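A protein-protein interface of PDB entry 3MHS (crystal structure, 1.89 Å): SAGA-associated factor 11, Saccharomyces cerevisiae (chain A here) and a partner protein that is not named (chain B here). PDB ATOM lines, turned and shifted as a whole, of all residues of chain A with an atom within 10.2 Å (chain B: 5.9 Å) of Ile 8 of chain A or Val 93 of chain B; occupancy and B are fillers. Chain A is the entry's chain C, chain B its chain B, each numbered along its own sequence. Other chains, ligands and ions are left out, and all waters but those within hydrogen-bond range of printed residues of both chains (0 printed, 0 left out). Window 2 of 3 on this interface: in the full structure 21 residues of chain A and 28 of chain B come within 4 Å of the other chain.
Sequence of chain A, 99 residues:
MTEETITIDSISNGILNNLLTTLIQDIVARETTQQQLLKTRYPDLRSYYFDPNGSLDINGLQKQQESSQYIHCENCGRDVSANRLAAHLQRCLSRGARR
The guanidinium group of Arg 86 of chain B lies within salt-bridge range of the side-chain carboxylate of Asp 9 of chain A, 2.9 Å away.
The side-chain hydroxyl (OG) of Ser 12 of chain A is in hydrogen-bond range of the backbone carbonyl oxygen (O) of Ile 8 of chain A (2.6 Å).
Ile 8 of chain A touches Arg 86 of chain B. Ile 8 of chain A touches Leu 89 of chain B (CD1 to CB, 3.8 Å). CG2 of Val 93 of chain B touches CD1 of Ile 8 of chain A (3.3 Å). Ile 11 of chain A touches Ile 12 of chain B. Leu 89 of chain B touches Ile 11 of chain A. CG2 of Ile 85 of chain B touches OG of Ser 12 of chain A (3.7 Å). Ser 12 of chain A touches Arg 86 of chain B. Ser 12 of chain A touches Leu 89 of chain B. Arg 86 of chain B touches Asn 13 of chain A (NH2 to OD1, 3.9 Å). Ile 15 of chain A touches Ile 85 of chain B.
Of the printed residues of chain B, Ile 8 of chain A touches Arg 86, Leu 89 and Val 93. Printed residues of chain A within 4 Å of Ile 12 of chain B: Ile 11. Of the printed residues of chain A, Arg 86 of chain B touches Ile 8 (3.5 Å), Asp 9 (2.9 Å), Ser 12 (3.1 Å) and Asn 13 (3.9 Å). Of the printed residues of chain A, Leu 89 of chain B touches Ile 8, Ile 11 and Ser 12. Val 93 of chain B touches just one residue of chain A: Ile 8. No residue of chain A comes within 4 Å of Asp 94 of chain B.
Of the 11 printed residues of chain B, 5 touch a printed residue of chain A. Hydrophobic or aromatic side chains of chain B within 4 Å of the printed part of chain A: Ile 12, Ile 85, Leu 89 and Val 93. Along chain B the printed residues that touch a printed residue of chain A span positions 12 to 93. Of the 12 printed residues of chain A, 6 touch a printed residue of chain B. Hydrophobic or aromatic side chains of chain A within 4 Å of the printed part of chain B: Ile 8, Ile 11 and Ile 15. Among the printed residues, 11 pairs touch across the chains.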
ATOM      1  N   THR A   5     -13.305 -22.233  28.261  1.00  0.00           N
ATOM      2  CA  THR A   5     -11.911 -22.628  28.453  1.00  0.00           C
ATOM      3  C   THR A   5     -11.058 -22.299  27.227  1.00  0.00           C
ATOM      4  O   THR A   5     -11.501 -22.465  26.088  1.00  0.00           O
ATOM      5  CB  THR A   5     -11.807 -24.147  28.719  1.00  0.00           C
ATOM      6  OG1 THR A   5     -12.762 -24.531  29.721  1.00  0.00           O
ATOM      7  CG2 THR A   5     -10.400 -24.519  29.171  1.00  0.00           C
ATOM      8  N   ILE A   6      -9.834 -21.842  27.474  1.00  0.00           N
ATOM      9  CA  ILE A   6      -8.925 -21.504  26.394  1.00  0.00           C
ATOM     10  C   ILE A   6      -7.821 -22.554  26.299  1.00  0.00           C
ATOM     11  O   ILE A   6      -7.180 -22.906  27.300  1.00  0.00           O
ATOM     12  CB  ILE A   6      -8.352 -20.064  26.537  1.00  0.00           C
ATOM     13  CG1 ILE A   6      -7.329 -19.977  27.686  1.00  0.00           C
ATOM     14  CG2 ILE A   6      -9.501 -19.065  26.775  1.00  0.00           C
ATOM     15  CD1 ILE A   6      -6.168 -19.010  27.404  1.00  0.00           C
ATOM     16  N   THR A   7      -7.633 -23.060  25.083  1.00  0.00           N
ATOM     17  CA  THR A   7      -6.697 -24.134  24.802  1.00  0.00           C
ATOM     18  C   THR A   7      -5.917 -23.799  23.522  1.00  0.00           C
ATOM     19  O   THR A   7      -6.395 -23.037  22.675  1.00  0.00           O
ATOM     20  CB  THR A   7      -7.465 -25.457  24.550  1.00  0.00           C
ATOM     21  OG1 THR A   7      -8.341 -25.300  23.418  1.00  0.00           O
ATOM     22  CG2 THR A   7      -8.287 -25.849  25.773  1.00  0.00           C
ATOM     23  N   ILE A   8      -4.731 -24.387  23.380  1.00  0.00           N
ATOM     24  CA  ILE A   8      -3.979 -24.302  22.132  1.00  0.00           C
ATOM     25  C   ILE A   8      -4.936 -24.567  20.958  1.00  0.00           C
ATOM     26  O   ILE A   8      -4.966 -23.795  20.006  1.00  0.00           O
ATOM     27  CB  ILE A   8      -2.783 -25.283  22.112  1.00  0.00           C
ATOM     28  CG1 ILE A   8      -1.818 -25.003  23.277  1.00  0.00           C
ATOM     29  CG2 ILE A   8      -1.997 -25.176  20.802  1.00  0.00           C
ATOM     30  CD1 ILE A   8      -0.909 -23.816  23.075  1.00  0.00           C
ATOM     31  N   ASP A   9      -5.743 -25.624  21.031  1.00  0.00           N
ATOM     32  CA  ASP A   9      -6.723 -25.892  19.971  1.00  0.00           C
ATOM     33  C   ASP A   9      -7.701 -24.719  19.719  1.00  0.00           C
ATOM     34  O   ASP A   9      -7.976 -24.366  18.557  1.00  0.00           O
ATOM     35  CB  ASP A   9      -7.499 -27.178  20.254  1.00  0.00           C
ATOM     36  CG  ASP A   9      -6.722 -28.432  19.875  1.00  0.00           C
ATOM     37  OD1 ASP A   9      -5.481 -28.365  19.735  1.00  0.00           O
ATOM     38  OD2 ASP A   9      -7.363 -29.494  19.725  1.00  0.00           O
ATOM     39  N   SER A  10      -8.227 -24.122  20.793  1.00  0.00           N
ATOM     40  CA  SER A  10      -9.186 -23.010  20.672  1.00  0.00           C
ATOM     41  C   SER A  10      -8.514 -21.752  20.125  1.00  0.00           C
ATOM     42  O   SER A  10      -9.014 -21.149  19.170  1.00  0.00           O
ATOM     43  CB  SER A  10      -9.888 -22.701  22.012  1.00  0.00           C
ATOM     44  OG  SER A  10      -9.052 -21.991  22.921  1.00  0.00           O
ATOM     45  N   ILE A  11      -7.393 -21.361  20.721  1.00  0.00           N
ATOM     46  CA  ILE A  11      -6.681 -20.173  20.261  1.00  0.00           C
ATOM     47  C   ILE A  11      -6.183 -20.344  18.821  1.00  0.00           C
ATOM     48  O   ILE A  11      -6.215 -19.406  18.039  1.00  0.00           O
ATOM     49  CB  ILE A  11      -5.474 -19.826  21.141  1.00  0.00           C
ATOM     50  CG1 ILE A  11      -5.924 -19.094  22.399  1.00  0.00           C
ATOM     51  CG2 ILE A  11      -4.533 -18.927  20.365  1.00  0.00           C
ATOM     52  CD1 ILE A  11      -4.776 -18.627  23.263  1.00  0.00           C
ATOM     53  N   SER A  12      -5.736 -21.546  18.487  1.00  0.00           N
ATOM     54  CA  SER A  12      -5.247 -21.841  17.151  1.00  0.00           C
ATOM     55  C   SER A  12      -6.378 -21.732  16.144  1.00  0.00           C
ATOM     56  O   SER A  12      -6.188 -21.188  15.053  1.00  0.00           O
ATOM     57  CB  SER A  12      -4.652 -23.234  17.119  1.00  0.00           C
ATOM     58  OG  SER A  12      -3.501 -23.254  17.920  1.00  0.00           O
ATOM     59  N   ASN A  13      -7.555 -22.227  16.529  1.00  0.00           N
ATOM     60  CA  ASN A  13      -8.742 -22.145  15.685  1.00  0.00           C
ATOM     61  C   ASN A  13      -9.093 -20.680  15.452  1.00  0.00           C
ATOM     62  O   ASN A  13      -9.553 -20.315  14.373  1.00  0.00           O
ATOM     63  CB  ASN A  13      -9.942 -22.877  16.311  1.00  0.00           C
ATOM     64  CG  ASN A  13      -9.765 -24.397  16.346  1.00  0.00           C
ATOM     65  OD1 ASN A  13      -9.544 -25.036  15.317  1.00  0.00           O
ATOM     66  ND2 ASN A  13      -9.904 -24.983  17.541  1.00  0.00           N
ATOM     67  N   GLY A  14      -8.874 -19.854  16.474  1.00  0.00           N
ATOM     68  CA  GLY A  14      -9.165 -18.428  16.397  1.00  0.00           C
ATOM     69  C   GLY A  14      -8.168 -17.719  15.490  1.00  0.00           C
ATOM     70  O   GLY A  14      -8.520 -16.797  14.769  1.00  0.00           O
ATOM     71  N   ILE A  15      -6.913 -18.139  15.553  1.00  0.00           N
ATOM     72  CA  ILE A  15      -5.892 -17.574  14.684  1.00  0.00           C
ATOM     73  C   ILE A  15      -6.227 -17.928  13.251  1.00  0.00           C
ATOM     74  O   ILE A  15      -6.246 -17.054  12.407  1.00  0.00           O
ATOM     75  CB  ILE A  15      -4.486 -18.016  15.100  1.00  0.00           C
ATOM     76  CG1 ILE A  15      -4.090 -17.247  16.369  1.00  0.00           C
ATOM     77  CG2 ILE A  15      -3.470 -17.786  13.922  1.00  0.00           C
ATOM     78  CD1 ILE A  15      -2.885 -17.811  17.134  1.00  0.00           C
ATOM     79  N   LEU A  16      -6.567 -19.187  12.989  1.00  0.00           N
ATOM     80  CA  LEU A  16      -6.945 -19.621  11.643  1.00  0.00           C
ATOM     81  C   LEU A  16      -8.201 -18.902  11.186  1.00  0.00           C
ATOM     82  O   LEU A  16      -8.265 -18.428  10.057  1.00  0.00           O
ATOM     83  CB  LEU A  16      -7.151 -21.136  11.574  1.00  0.00           C
ATOM     84  CG  LEU A  16      -7.569 -21.733  10.221  1.00  0.00           C
ATOM     85  CD1 LEU A  16      -6.477 -21.559   9.182  1.00  0.00           C
ATOM     86  CD2 LEU A  16      -7.967 -23.217  10.345  1.00  0.00           C
ATOM     87  N   ILE B  12      -0.566 -13.043  22.151  1.00  0.00           N
ATOM     88  CA  ILE B  12      -0.032 -14.157  21.384  1.00  0.00           C
ATOM     89  C   ILE B  12       0.209 -13.782  19.913  1.00  0.00           C
ATOM     90  O   ILE B  12       1.249 -14.106  19.358  1.00  0.00           O
ATOM     91  CB  ILE B  12      -0.969 -15.390  21.494  1.00  0.00           C
ATOM     92  CG1 ILE B  12      -0.904 -15.958  22.925  1.00  0.00           C
ATOM     93  CG2 ILE B  12      -0.621 -16.442  20.420  1.00  0.00           C
ATOM     94  CD1 ILE B  12      -1.899 -17.078  23.219  1.00  0.00           C
ATOM     95  N   ILE B  85       0.328 -23.805  13.446  1.00  0.00           N
ATOM     96  CA  ILE B  85       0.019 -22.798  14.485  1.00  0.00           C
ATOM     97  C   ILE B  85       0.250 -23.373  15.900  1.00  0.00           C
ATOM     98  O   ILE B  85       0.875 -22.740  16.754  1.00  0.00           O
ATOM     99  CB  ILE B  85      -1.424 -22.246  14.341  1.00  0.00           C
ATOM    100  CG1 ILE B  85      -1.612 -21.554  12.984  1.00  0.00           C
ATOM    101  CG2 ILE B  85      -1.735 -21.200  15.443  1.00  0.00           C
ATOM    102  CD1 ILE B  85      -3.069 -21.405  12.566  1.00  0.00           C
ATOM    103  N   ARG B  86      -0.213 -24.591  16.127  1.00  0.00           N
ATOM    104  CA  ARG B  86      -0.123 -25.163  17.466  1.00  0.00           C
ATOM    105  C   ARG B  86       1.337 -25.380  17.870  1.00  0.00           C
ATOM    106  O   ARG B  86       1.688 -25.122  19.005  1.00  0.00           O
ATOM    107  CB  ARG B  86      -0.954 -26.441  17.560  1.00  0.00           C
ATOM    108  CG  ARG B  86      -2.444 -26.173  17.458  1.00  0.00           C
ATOM    109  CD  ARG B  86      -3.247 -27.439  17.237  1.00  0.00           C
ATOM    110  NE  ARG B  86      -4.680 -27.162  17.181  1.00  0.00           N
ATOM    111  CZ  ARG B  86      -5.563 -27.943  16.572  1.00  0.00           C
ATOM    112  NH1 ARG B  86      -5.160 -29.057  15.974  1.00  0.00           N
ATOM    113  NH2 ARG B  86      -6.846 -27.609  16.556  1.00  0.00           N
ATOM    114  N   GLU B  87       2.186 -25.790  16.917  1.00  0.00           N
ATOM    115  CA  GLU B  87       3.627 -25.950  17.163  1.00  0.00           C
ATOM    116  C   GLU B  87       4.257 -24.613  17.552  1.00  0.00           C
ATOM    117  O   GLU B  87       5.083 -24.561  18.461  1.00  0.00           O
ATOM    118  CB  GLU B  87       4.357 -26.512  15.922  1.00  0.00           C
ATOM    119  CG  GLU B  87       4.110 -28.006  15.621  1.00  0.00           C
ATOM    120  CD  GLU B  87       4.636 -28.443  14.233  1.00  0.00           C
ATOM    121  OE1 GLU B  87       4.638 -29.669  13.949  1.00  0.00           O
ATOM    122  OE2 GLU B  87       5.038 -27.567  13.421  1.00  0.00           O
ATOM    123  N   LEU B  89       2.620 -22.099  18.841  1.00  0.00           N
ATOM    124  CA  LEU B  89       2.005 -21.718  20.129  1.00  0.00           C
ATOM    125  C   LEU B  89       2.607 -22.496  21.303  1.00  0.00           C
ATOM    126  O   LEU B  89       2.883 -21.930  22.357  1.00  0.00           O
ATOM    127  CB  LEU B  89       0.493 -21.960  20.103  1.00  0.00           C
ATOM    128  CG  LEU B  89      -0.371 -20.966  19.331  1.00  0.00           C
ATOM    129  CD1 LEU B  89      -1.828 -21.243  19.623  1.00  0.00           C
ATOM    130  CD2 LEU B  89      -0.005 -19.542  19.709  1.00  0.00           C
ATOM    131  N   GLU B  90       2.791 -23.799  21.116  1.00  0.00           N
ATOM    132  CA  GLU B  90       3.411 -24.661  22.136  1.00  0.00           C
ATOM    133  C   GLU B  90       4.844 -24.241  22.465  1.00  0.00           C
ATOM    134  O   GLU B  90       5.418 -24.681  23.454  1.00  0.00           O
ATOM    135  CB  GLU B  90       3.370 -26.124  21.689  1.00  0.00           C
ATOM    136  CG  GLU B  90       1.943 -26.684  21.663  1.00  0.00           C
ATOM    137  CD  GLU B  90       1.876 -28.155  21.293  1.00  0.00           C
ATOM    138  OE1 GLU B  90       2.513 -28.552  20.282  1.00  0.00           O
ATOM    139  OE2 GLU B  90       1.165 -28.903  22.006  1.00  0.00           O
ATOM    140  N   GLU B  91       5.394 -23.364  21.641  1.00  0.00           N
ATOM    141  CA  GLU B  91       6.708 -22.778  21.870  1.00  0.00           C
ATOM    142  C   GLU B  91       6.626 -21.806  23.045  1.00  0.00           C
ATOM    143  O   GLU B  91       7.415 -21.906  23.980  1.00  0.00           O
ATOM    144  CB  GLU B  91       7.165 -22.035  20.606  1.00  0.00           C
ATOM    145  CG  GLU B  91       8.619 -22.230  20.187  1.00  0.00           C
ATOM    146  CD  GLU B  91       8.771 -22.324  18.669  1.00  0.00           C
ATOM    147  OE1 GLU B  91       8.957 -21.288  17.997  1.00  0.00           O
ATOM    148  OE2 GLU B  91       8.667 -23.439  18.130  1.00  0.00           O
ATOM    149  N   ILE B  92       5.639 -20.904  23.020  1.00  0.00           N
ATOM    150  CA  ILE B  92       5.636 -19.753  23.938  1.00  0.00           C
ATOM    151  C   ILE B  92       4.447 -19.580  24.889  1.00  0.00           C
ATOM    152  O   ILE B  92       4.245 -18.503  25.444  1.00  0.00           O
ATOM    153  CB  ILE B  92       5.875 -18.443  23.165  1.00  0.00           C
ATOM    154  CG1 ILE B  92       4.761 -18.203  22.140  1.00  0.00           C
ATOM    155  CG2 ILE B  92       7.243 -18.494  22.522  1.00  0.00           C
ATOM    156  CD1 ILE B  92       3.780 -17.114  22.522  1.00  0.00           C
ATOM    157  N   VAL B  93       3.703 -20.651  25.135  1.00  0.00           N
ATOM    158  CA  VAL B  93       2.738 -20.645  26.219  1.00  0.00           C
ATOM    159  C   VAL B  93       2.975 -21.820  27.176  1.00  0.00           C
ATOM    160  O   VAL B  93       3.331 -22.925  26.756  1.00  0.00           O
ATOM    161  CB  VAL B  93       1.289 -20.694  25.709  1.00  0.00           C
ATOM    162  CG1 VAL B  93       1.013 -19.536  24.750  1.00  0.00           C
ATOM    163  CG2 VAL B  93       0.983 -22.043  25.075  1.00  0.00           C
ATOM    164  N   ASP B  94       2.799 -21.568  28.468  1.00  0.00           N
ATOM    165  CA  ASP B  94       2.798 -22.639  29.445  1.00  0.00           C
ATOM    166  C   ASP B  94       1.370 -23.145  29.529  1.00  0.00           C
ATOM    167  O   ASP B  94       0.438 -22.345  29.528  1.00  0.00           O
ATOM    168  CB  ASP B  94       3.245 -22.113  30.809  1.00  0.00           C
ATOM    169  CG  ASP B  94       4.550 -21.336  30.742  1.00  0.00           C
ATOM    170  OD1 ASP B  94       5.549 -21.904  30.243  1.00  0.00           O
ATOM    171  OD2 ASP B  94       4.577 -20.170  31.205  1.00  0.00           O
ATOM    172  N   THR B  95       1.183 -24.460  29.577  1.00  0.00           N
ATOM    173  CA  THR B  95      -0.151 -25.021  29.823  1.00  0.00           C
ATOM    174  C   THR B  95      -0.173 -25.892  31.084  1.00  0.00           C
ATOM    175  O   THR B  95       0.671 -25.750  31.969  1.00  0.00           O
ATOM    176  CB  THR B  95      -0.671 -25.846  28.614  1.00  0.00           C
ATOM    177  OG1 THR B  95      -0.208 -27.198  28.705  1.00  0.00           O
ATOM    178  CG2 THR B  95      -0.232 -25.220  27.273  1.00  0.00           C
